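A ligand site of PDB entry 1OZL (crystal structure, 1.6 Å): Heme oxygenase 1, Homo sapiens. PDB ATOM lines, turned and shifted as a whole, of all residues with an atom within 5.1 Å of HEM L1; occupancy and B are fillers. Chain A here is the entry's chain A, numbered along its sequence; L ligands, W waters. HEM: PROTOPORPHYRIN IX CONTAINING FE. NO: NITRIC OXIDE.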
ATOM      1  N   SER A  14      23.299  -6.718  -1.446  1.00  0.00           N
ATOM      2  CA  SER A  14      23.489  -5.685  -2.471  1.00  0.00           C
ATOM      3  C   SER A  14      24.691  -4.807  -2.129  1.00  0.00           C
ATOM      4  O   SER A  14      25.500  -4.489  -3.003  1.00  0.00           O
ATOM      5  CB  SER A  14      22.231  -4.827  -2.592  1.00  0.00           C
ATOM      6  OG  SER A  14      21.956  -4.135  -1.378  1.00  0.00           O
ATOM      7  N   LYS A  18      28.496  -4.676  -4.030  1.00  0.00           N
ATOM      8  CA  LYS A  18      29.052  -3.408  -4.486  1.00  0.00           C
ATOM      9  C   LYS A  18      30.456  -3.179  -3.923  1.00  0.00           C
ATOM     10  O   LYS A  18      31.391  -2.851  -4.653  1.00  0.00           O
ATOM     11  CB  LYS A  18      28.141  -2.257  -4.077  1.00  0.00           C
ATOM     12  CG  LYS A  18      28.569  -0.895  -4.602  1.00  0.00           C
ATOM     13  CD  LYS A  18      27.594   0.188  -4.180  1.00  0.00           C
ATOM     14  CE  LYS A  18      28.008   1.545  -4.721  1.00  0.00           C
ATOM     15  NZ  LYS A  18      28.002   1.577  -6.208  1.00  0.00           N
ATOM     16  N   HIS A  25      35.960  -3.658 -10.594  1.00  0.00           N
ATOM     17  CA  HIS A  25      35.259  -2.733 -11.469  1.00  0.00           C
ATOM     18  C   HIS A  25      36.291  -1.718 -11.971  1.00  0.00           C
ATOM     19  O   HIS A  25      36.320  -1.382 -13.149  1.00  0.00           O
ATOM     20  CB  HIS A  25      34.126  -2.015 -10.742  1.00  0.00           C
ATOM     21  CG  HIS A  25      33.269  -1.163 -11.630  1.00  0.00           C
ATOM     22  ND1 HIS A  25      33.677   0.076 -12.103  1.00  0.00           N
ATOM     23  CD2 HIS A  25      32.042  -1.375 -12.156  1.00  0.00           C
ATOM     24  CE1 HIS A  25      32.740   0.572 -12.885  1.00  0.00           C
ATOM     25  NE2 HIS A  25      31.733  -0.291 -12.943  1.00  0.00           N
ATOM     26  N   ALA A  28      38.399  -3.135 -14.542  1.00  0.00           N
ATOM     27  CA  ALA A  28      37.701  -3.128 -15.826  1.00  0.00           C
ATOM     28  C   ALA A  28      37.819  -1.750 -16.456  1.00  0.00           C
ATOM     29  O   ALA A  28      38.034  -1.626 -17.663  1.00  0.00           O
ATOM     30  CB  ALA A  28      36.225  -3.501 -15.626  1.00  0.00           C
ATOM     31  N   GLU A  29      37.664  -0.707 -15.647  1.00  0.00           N
ATOM     32  CA  GLU A  29      37.769   0.668 -16.141  1.00  0.00           C
ATOM     33  C   GLU A  29      39.190   0.927 -16.628  1.00  0.00           C
ATOM     34  O   GLU A  29      39.401   1.744 -17.527  1.00  0.00           O
ATOM     35  CB  GLU A  29      37.453   1.669 -15.025  1.00  0.00           C
ATOM     36  CG  GLU A  29      36.017   1.661 -14.518  1.00  0.00           C
ATOM     37  CD  GLU A  29      35.823   2.606 -13.355  1.00  0.00           C
ATOM     38  OE1 GLU A  29      35.954   3.843 -13.553  1.00  0.00           O
ATOM     39  OE2 GLU A  29      35.547   2.133 -12.242  1.00  0.00           O
ATOM     40  N   MET A  34      39.019  -0.589 -22.596  1.00  0.00           N
ATOM     41  CA  MET A  34      38.071   0.332 -21.986  1.00  0.00           C
ATOM     42  C   MET A  34      38.650   1.724 -21.790  1.00  0.00           C
ATOM     43  O   MET A  34      37.905   2.707 -21.762  1.00  0.00           O
ATOM     44  CB  MET A  34      37.560  -0.231 -20.660  1.00  0.00           C
ATOM     45  CG  MET A  34      36.546  -1.355 -20.820  1.00  0.00           C
ATOM     46  SD  MET A  34      35.026  -0.798 -21.617  1.00  0.00           S
ATOM     47  CE  MET A  34      35.296  -1.260 -23.279  1.00  0.00           C
ATOM     48  N   GLN A  38      36.768   5.008 -23.137  1.00  0.00           N
ATOM     49  CA  GLN A  38      36.456   6.191 -22.329  1.00  0.00           C
ATOM     50  C   GLN A  38      37.120   7.446 -22.887  1.00  0.00           C
ATOM     51  O   GLN A  38      36.600   8.552 -22.717  1.00  0.00           O
ATOM     52  CB  GLN A  38      36.892   5.952 -20.886  1.00  0.00           C
ATOM     53  CG  GLN A  38      36.181   4.769 -20.233  1.00  0.00           C
ATOM     54  CD  GLN A  38      36.679   4.481 -18.843  1.00  0.00           C
ATOM     55  OE1 GLN A  38      36.397   5.231 -17.899  1.00  0.00           O
ATOM     56  NE2 GLN A  38      37.430   3.388 -18.693  1.00  0.00           N
ATOM     57  N   TYR A 114      33.185 -17.027 -21.267  1.00  0.00           N
ATOM     58  CA  TYR A 114      32.156 -16.359 -20.475  1.00  0.00           C
ATOM     59  C   TYR A 114      30.832 -17.133 -20.594  1.00  0.00           C
ATOM     60  O   TYR A 114      30.192 -17.444 -19.592  1.00  0.00           O
ATOM     61  CB  TYR A 114      31.967 -14.924 -20.985  1.00  0.00           C
ATOM     62  CG  TYR A 114      31.394 -13.928 -20.007  1.00  0.00           C
ATOM     63  CD1 TYR A 114      30.476 -14.310 -19.013  1.00  0.00           C
ATOM     64  CD2 TYR A 114      31.710 -12.571 -20.108  1.00  0.00           C
ATOM     65  CE1 TYR A 114      29.890 -13.364 -18.170  1.00  0.00           C
ATOM     66  CE2 TYR A 114      31.128 -11.616 -19.271  1.00  0.00           C
ATOM     67  CZ  TYR A 114      30.223 -12.014 -18.309  1.00  0.00           C
ATOM     68  OH  TYR A 114      29.647 -11.065 -17.495  1.00  0.00           O
ATOM     69  N   TYR A 134      23.260  -9.713 -11.475  1.00  0.00           N
ATOM     70  CA  TYR A 134      23.643  -8.464 -10.810  1.00  0.00           C
ATOM     71  C   TYR A 134      24.665  -7.698 -11.635  1.00  0.00           C
ATOM     72  O   TYR A 134      24.467  -6.529 -11.958  1.00  0.00           O
ATOM     73  CB  TYR A 134      24.231  -8.746  -9.430  1.00  0.00           C
ATOM     74  CG  TYR A 134      25.083  -7.615  -8.859  1.00  0.00           C
ATOM     75  CD1 TYR A 134      24.502  -6.424  -8.418  1.00  0.00           C
ATOM     76  CD2 TYR A 134      26.471  -7.734  -8.801  1.00  0.00           C
ATOM     77  CE1 TYR A 134      25.286  -5.380  -7.919  1.00  0.00           C
ATOM     78  CE2 TYR A 134      27.263  -6.694  -8.303  1.00  0.00           C
ATOM     79  CZ  TYR A 134      26.665  -5.515  -7.872  1.00  0.00           C
ATOM     80  OH  TYR A 134      27.458  -4.493  -7.399  1.00  0.00           O
ATOM     81  N   THR A 135      25.769  -8.361 -11.953  1.00  0.00           N
ATOM     82  CA  THR A 135      26.843  -7.709 -12.708  1.00  0.00           C
ATOM     83  C   THR A 135      26.401  -7.211 -14.079  1.00  0.00           C
ATOM     84  O   THR A 135      26.792  -6.115 -14.491  1.00  0.00           O
ATOM     85  CB  THR A 135      28.052  -8.648 -12.860  1.00  0.00           C
ATOM     86  OG1 THR A 135      27.631  -9.901 -13.427  1.00  0.00           O
ATOM     87  CG2 THR A 135      28.680  -8.911 -11.505  1.00  0.00           C
ATOM     88  N   ARG A 136      25.579  -7.996 -14.782  1.00  0.00           N
ATOM     89  CA  ARG A 136      25.126  -7.576 -16.105  1.00  0.00           C
ATOM     90  C   ARG A 136      24.062  -6.478 -16.044  1.00  0.00           C
ATOM     91  O   ARG A 136      24.271  -5.377 -16.539  1.00  0.00           O
ATOM     92  CB  ARG A 136      24.563  -8.763 -16.899  1.00  0.00           C
ATOM     93  CG  ARG A 136      25.530  -9.883 -17.214  1.00  0.00           C
ATOM     94  CD  ARG A 136      26.903  -9.403 -17.653  1.00  0.00           C
ATOM     95  NE  ARG A 136      26.888  -8.320 -18.635  1.00  0.00           N
ATOM     96  CZ  ARG A 136      27.985  -7.882 -19.243  1.00  0.00           C
ATOM     97  NH1 ARG A 136      29.160  -8.449 -18.957  1.00  0.00           N
ATOM     98  NH2 ARG A 136      27.936  -6.867 -20.104  1.00  0.00           N
ATOM     99  N   LEU A 138      22.514  -4.694 -13.319  1.00  0.00           N
ATOM    100  CA  LEU A 138      22.707  -3.500 -12.511  1.00  0.00           C
ATOM    101  C   LEU A 138      23.827  -2.657 -13.114  1.00  0.00           C
ATOM    102  O   LEU A 138      23.798  -1.431 -13.036  1.00  0.00           O
ATOM    103  CB  LEU A 138      23.048  -3.872 -11.056  1.00  0.00           C
ATOM    104  CG  LEU A 138      22.047  -3.275 -10.055  1.00  0.00           C
ATOM    105  CD1 LEU A 138      20.674  -3.837 -10.360  1.00  0.00           C
ATOM    106  CD2 LEU A 138      22.458  -3.609  -8.634  1.00  0.00           C
ATOM    107  N   GLY A 139      24.798  -3.315 -13.723  1.00  0.00           N
ATOM    108  CA  GLY A 139      25.877  -2.581 -14.359  1.00  0.00           C
ATOM    109  C   GLY A 139      25.369  -1.782 -15.541  1.00  0.00           C
ATOM    110  O   GLY A 139      25.677  -0.604 -15.682  1.00  0.00           O
ATOM    111  N   SER A 142      23.310   1.092 -14.374  1.00  0.00           N
ATOM    112  CA  SER A 142      24.046   2.143 -13.671  1.00  0.00           C
ATOM    113  C   SER A 142      24.936   2.973 -14.595  1.00  0.00           C
ATOM    114  O   SER A 142      24.804   4.194 -14.658  1.00  0.00           O
ATOM    115  CB  SER A 142      24.891   1.533 -12.555  1.00  0.00           C
ATOM    116  OG  SER A 142      24.090   0.842 -11.620  1.00  0.00           O
ATOM    117  N   GLY A 143      25.837   2.303 -15.317  1.00  0.00           N
ATOM    118  CA  GLY A 143      26.731   3.017 -16.201  1.00  0.00           C
ATOM    119  C   GLY A 143      26.375   2.934 -17.671  1.00  0.00           C
ATOM    120  O   GLY A 143      27.142   3.373 -18.525  1.00  0.00           O
ATOM    121  N   VAL A 146      26.184   6.434 -19.334  1.00  0.00           N
ATOM    122  CA  VAL A 146      27.507   7.022 -19.518  1.00  0.00           C
ATOM    123  C   VAL A 146      28.206   6.405 -20.727  1.00  0.00           C
ATOM    124  O   VAL A 146      28.710   7.111 -21.593  1.00  0.00           O
ATOM    125  CB  VAL A 146      28.406   6.790 -18.273  1.00  0.00           C
ATOM    126  CG1 VAL A 146      29.816   7.294 -18.546  1.00  0.00           C
ATOM    127  CG2 VAL A 146      27.817   7.500 -17.070  1.00  0.00           C
ATOM    128  N   LEU A 147      28.210   5.074 -20.786  1.00  0.00           N
ATOM    129  CA  LEU A 147      28.835   4.351 -21.875  1.00  0.00           C
ATOM    130  C   LEU A 147      28.156   4.596 -23.213  1.00  0.00           C
ATOM    131  O   LEU A 147      28.816   4.649 -24.258  1.00  0.00           O
ATOM    132  CB  LEU A 147      28.875   2.864 -21.547  1.00  0.00           C
ATOM    133  CG  LEU A 147      29.633   2.537 -20.261  1.00  0.00           C
ATOM    134  CD1 LEU A 147      29.399   1.091 -19.851  1.00  0.00           C
ATOM    135  CD2 LEU A 147      31.121   2.795 -20.472  1.00  0.00           C
ATOM    136  N   LYS A 179      16.371   0.121  -9.534  1.00  0.00           N
ATOM    137  CA  LYS A 179      17.599  -0.347  -8.891  1.00  0.00           C
ATOM    138  C   LYS A 179      17.373  -0.589  -7.400  1.00  0.00           C
ATOM    139  O   LYS A 179      17.939  -1.514  -6.825  1.00  0.00           O
ATOM    140  CB  LYS A 179      18.733   0.668  -9.093  1.00  0.00           C
ATOM    141  CG  LYS A 179      19.287   0.700 -10.508  1.00  0.00           C
ATOM    142  CD  LYS A 179      20.431   1.703 -10.647  1.00  0.00           C
ATOM    143  CE  LYS A 179      21.621   1.326  -9.767  1.00  0.00           C
ATOM    144  NZ  LYS A 179      22.731   2.317  -9.852  1.00  0.00           N
ATOM    145  N   ARG A 183      17.638  -4.261  -5.737  1.00  0.00           N
ATOM    146  CA  ARG A 183      18.531  -4.465  -4.601  1.00  0.00           C
ATOM    147  C   ARG A 183      17.743  -5.070  -3.444  1.00  0.00           C
ATOM    148  O   ARG A 183      18.230  -5.949  -2.737  1.00  0.00           O
ATOM    149  CB  ARG A 183      19.155  -3.134  -4.172  1.00  0.00           C
ATOM    150  CG  ARG A 183      20.197  -2.629  -5.157  1.00  0.00           C
ATOM    151  CD  ARG A 183      20.705  -1.252  -4.786  1.00  0.00           C
ATOM    152  NE  ARG A 183      21.764  -0.820  -5.700  1.00  0.00           N
ATOM    153  CZ  ARG A 183      22.174   0.435  -5.836  1.00  0.00           C
ATOM    154  NH1 ARG A 183      21.619   1.397  -5.120  1.00  0.00           N
ATOM    155  NH2 ARG A 183      23.136   0.725  -6.698  1.00  0.00           N
ATOM    156  N   ALA A 206      32.832 -12.730 -12.680  1.00  0.00           N
ATOM    157  CA  ALA A 206      32.159 -12.148 -13.827  1.00  0.00           C
ATOM    158  C   ALA A 206      33.007 -11.000 -14.376  1.00  0.00           C
ATOM    159  O   ALA A 206      33.249 -10.913 -15.583  1.00  0.00           O
ATOM    160  CB  ALA A 206      30.773 -11.653 -13.438  1.00  0.00           C
ATOM    161  N   PHE A 207      33.466 -10.121 -13.494  1.00  0.00           N
ATOM    162  CA  PHE A 207      34.296  -9.006 -13.934  1.00  0.00           C
ATOM    163  C   PHE A 207      35.571  -9.525 -14.607  1.00  0.00           C
ATOM    164  O   PHE A 207      35.972  -9.031 -15.653  1.00  0.00           O
ATOM    165  CB  PHE A 207      34.683  -8.098 -12.757  1.00  0.00           C
ATOM    166  CG  PHE A 207      33.616  -7.131 -12.371  1.00  0.00           C
ATOM    167  CD1 PHE A 207      32.596  -7.500 -11.493  1.00  0.00           C
ATOM    168  CD2 PHE A 207      33.622  -5.828 -12.862  1.00  0.00           C
ATOM    169  CE1 PHE A 207      31.611  -6.593 -11.125  1.00  0.00           C
ATOM    170  CE2 PHE A 207      32.646  -4.925 -12.495  1.00  0.00           C
ATOM    171  CZ  PHE A 207      31.634  -5.299 -11.617  1.00  0.00           C
ATOM    172  N   ASN A 210      35.022 -10.607 -18.023  1.00  0.00           N
ATOM    173  CA  ASN A 210      34.842  -9.426 -18.872  1.00  0.00           C
ATOM    174  C   ASN A 210      36.202  -8.846 -19.230  1.00  0.00           C
ATOM    175  O   ASN A 210      36.460  -8.498 -20.386  1.00  0.00           O
ATOM    176  CB  ASN A 210      34.030  -8.354 -18.129  1.00  0.00           C
ATOM    177  CG  ASN A 210      32.543  -8.525 -18.290  1.00  0.00           C
ATOM    178  OD1 ASN A 210      31.941  -8.058 -19.266  1.00  0.00           O
ATOM    179  ND2 ASN A 210      31.919  -9.195 -17.332  1.00  0.00           N
ATOM    180  N   PHE A 214      37.985  -8.214 -22.764  1.00  0.00           N
ATOM    181  CA  PHE A 214      38.490  -6.913 -23.221  1.00  0.00           C
ATOM    182  C   PHE A 214      39.907  -7.058 -23.756  1.00  0.00           C
ATOM    183  O   PHE A 214      40.256  -6.467 -24.768  1.00  0.00           O
ATOM    184  CB  PHE A 214      38.502  -5.876 -22.083  1.00  0.00           C
ATOM    185  CG  PHE A 214      37.134  -5.447 -21.628  1.00  0.00           C
ATOM    186  CD1 PHE A 214      36.057  -5.423 -22.504  1.00  0.00           C
ATOM    187  CD2 PHE A 214      36.951  -5.023 -20.320  1.00  0.00           C
ATOM    188  CE1 PHE A 214      34.805  -4.976 -22.087  1.00  0.00           C
ATOM    189  CE2 PHE A 214      35.699  -4.579 -19.889  1.00  0.00           C
ATOM    190  CZ  PHE A 214      34.633  -4.552 -20.771  1.00  0.00           C
HETATM  191  CHA HEM L   1      28.140   0.681 -11.660  1.00  0.00           C
HETATM  192  CHB HEM L   1      30.592   3.021 -15.157  1.00  0.00           C
HETATM  193  CHC HEM L   1      32.348  -1.243 -16.686  1.00  0.00           C
HETATM  194  CHD HEM L   1      29.349  -3.563 -13.647  1.00  0.00           C
HETATM  195  C1A HEM L   1      28.676   1.682 -12.474  1.00  0.00           C
HETATM  196  C2A HEM L   1      28.399   3.096 -12.309  1.00  0.00           C
HETATM  197  C3A HEM L   1      29.042   3.745 -13.322  1.00  0.00           C
HETATM  198  C4A HEM L   1      29.713   2.737 -14.111  1.00  0.00           C
HETATM  199  CMA HEM L   1      29.064   5.254 -13.563  1.00  0.00           C
HETATM  200  CAA HEM L   1      27.478   3.737 -11.252  1.00  0.00           C
HETATM  201  CBA HEM L   1      28.031   3.729  -9.835  1.00  0.00           C
HETATM  202  CGA HEM L   1      27.006   4.180  -8.816  1.00  0.00           C
HETATM  203  O1A HEM L   1      25.941   3.542  -8.717  1.00  0.00           O
HETATM  204  O2A HEM L   1      27.275   5.175  -8.101  1.00  0.00           O
HETATM  205  C1B HEM L   1      31.351   2.062 -15.825  1.00  0.00           C
HETATM  206  C2B HEM L   1      32.382   2.372 -16.781  1.00  0.00           C
HETATM  207  C3B HEM L   1      32.926   1.191 -17.192  1.00  0.00           C
HETATM  208  C4B HEM L   1      32.190   0.133 -16.468  1.00  0.00           C
HETATM  209  CMB HEM L   1      32.825   3.773 -17.225  1.00  0.00           C
HETATM  210  CAB HEM L   1      34.026   1.036 -18.019  1.00  0.00           C
HETATM  211  CBB HEM L   1      34.073   1.538 -19.392  1.00  0.00           C
HETATM  212  C1C HEM L   1      31.614  -2.238 -16.035  1.00  0.00           C
HETATM  213  C2C HEM L   1      31.740  -3.671 -16.317  1.00  0.00           C
HETATM  214  C3C HEM L   1      30.819  -4.310 -15.525  1.00  0.00           C
HETATM  215  C4C HEM L   1      30.195  -3.275 -14.707  1.00  0.00           C
HETATM  216  CMC HEM L   1      32.737  -4.334 -17.267  1.00  0.00           C
HETATM  217  CAC HEM L   1      30.439  -5.663 -15.548  1.00  0.00           C
HETATM  218  CBC HEM L   1      31.349  -6.804 -15.484  1.00  0.00           C
HETATM  219  C1D HEM L   1      28.839  -2.600 -12.791  1.00  0.00           C
HETATM  220  C2D HEM L   1      27.991  -2.907 -11.648  1.00  0.00           C
HETATM  221  C3D HEM L   1      27.622  -1.730 -11.104  1.00  0.00           C
HETATM  222  C4D HEM L   1      28.283  -0.679 -11.881  1.00  0.00           C
HETATM  223  CMD HEM L   1      27.494  -4.279 -11.214  1.00  0.00           C
HETATM  224  CAD HEM L   1      26.625  -1.621  -9.951  1.00  0.00           C
HETATM  225  CBD HEM L   1      27.242  -1.143  -8.647  1.00  0.00           C
HETATM  226  CGD HEM L   1      26.274  -1.214  -7.476  1.00  0.00           C
HETATM  227  O1D HEM L   1      26.075  -2.323  -6.932  1.00  0.00           O
HETATM  228  O2D HEM L   1      25.709  -0.163  -7.117  1.00  0.00           O
HETATM  229  NA  HEM L   1      29.478   1.458 -13.592  1.00  0.00           N
HETATM  230  NB  HEM L   1      31.258   0.687 -15.598  1.00  0.00           N
HETATM  231  NC  HEM L   1      30.653  -2.002 -15.049  1.00  0.00           N
HETATM  232  ND  HEM L   1      29.018  -1.224 -12.928  1.00  0.00           N
HETATM  233 FE   HEM L   1      30.099  -0.264 -14.288  1.00  0.00          FE
HETATM  234  N    NO L   2      28.924  -0.157 -15.213  1.00  0.00           N
HETATM  235  O    NO L   2      28.457  -0.359 -16.256  1.00  0.00           O
HETATM  236  O   HOH W   1      28.633  -2.714 -17.714  1.00  0.00           O
HETATM  237  O   HOH W   2      24.343  -2.739  -4.864  1.00  0.00           O
HETATM  238  O   HOH W   3      29.884  -3.431  -8.596  1.00  0.00           O
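Residues that only touch HEM L1: Asn 210, Gly 139, Met 34, Leu 147, Ser 142, Phe 207, Gly 143, Thr 135, Gln 38, Ala 28 and Phe 214. Hydrophobic or aromatic side chains within 4 Å of HEM L1: His 25, Ala 28, Met 34, Tyr 134, Leu 147, Phe 207 and Phe 214. Within 4 Å of HEM L1: Lys 18, His 25, Ala 28, Met 34, Gln 38, Tyr 134, Thr 135, Gly 139, Ser 142, Gly 143, Leu 147, Lys 179, Arg 183, Phe 207, Asn 210 and Phe 214.
The side-chain hydroxyl of Ser 142 lies within hydrogen-bond range of the backbone carbonyl oxygen of Leu 138 (2.7 Å). The side-chain hydroxyl of Ser 142 is in hydrogen-bond range of the side-chain amino group of Lys 179, 2.7 Å away. The side-chain amide nitrogen of Asn 210 is in hydrogen-bond range of the backbone carbonyl oxygen of Ala 206. The side-chain amide oxygen (OD1) of Asn 210 sits at hydrogen-bond distance from the guanidinium group (NH1) of Arg 136, at 2.8 Å. NE2 of Gln 38 sits close to O of Met 34. The side-chain amide nitrogen of Asn 210 is in hydrogen-bond range of the side-chain hydroxyl of Tyr 114, 2.9 Å away. The side-chain carboxylate (OE2) of Glu 29 lies within hydrogen-bond range of a ring nitrogen (ND1) of His 25, 2.8 Å away. The side-chain amide nitrogen (NE2) of Gln 38 sits at hydrogen-bond distance from the backbone carbonyl oxygen (O) of Glu 29, at 2.8 Å.
A nitrogen (N) of NO L2 is bound to an iron atom (FE) of HEM L1, at 1.5 Å.
Water W2 lies within hydrogen-bond range of an oxygen (O1D) of HEM L1 (2.7 Å), the backbone carbonyl oxygen of Ser 14 (2.8 Å) and the guanidinium group of Arg 183 (3.3 Å).
NH2 of Arg 183 lies within salt-bridge range of O2D of HEM L1, 2.8 Å away. The side-chain amino group of Lys 179 lies within salt-bridge range of an oxygen (O1A) of HEM L1 (3.6 Å). The side-chain hydroxyl of Tyr 134 lies within hydrogen-bond range of an oxygen (O1D) of HEM L1, 2.6 Å away. The side-chain amino group (NZ) of Lys 18 is in salt-bridge range of an oxygen (O2D) of HEM L1, at 3.0 Å. NE2 of His 25 is bound to FE of HEM L1, at 2.1 Å.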
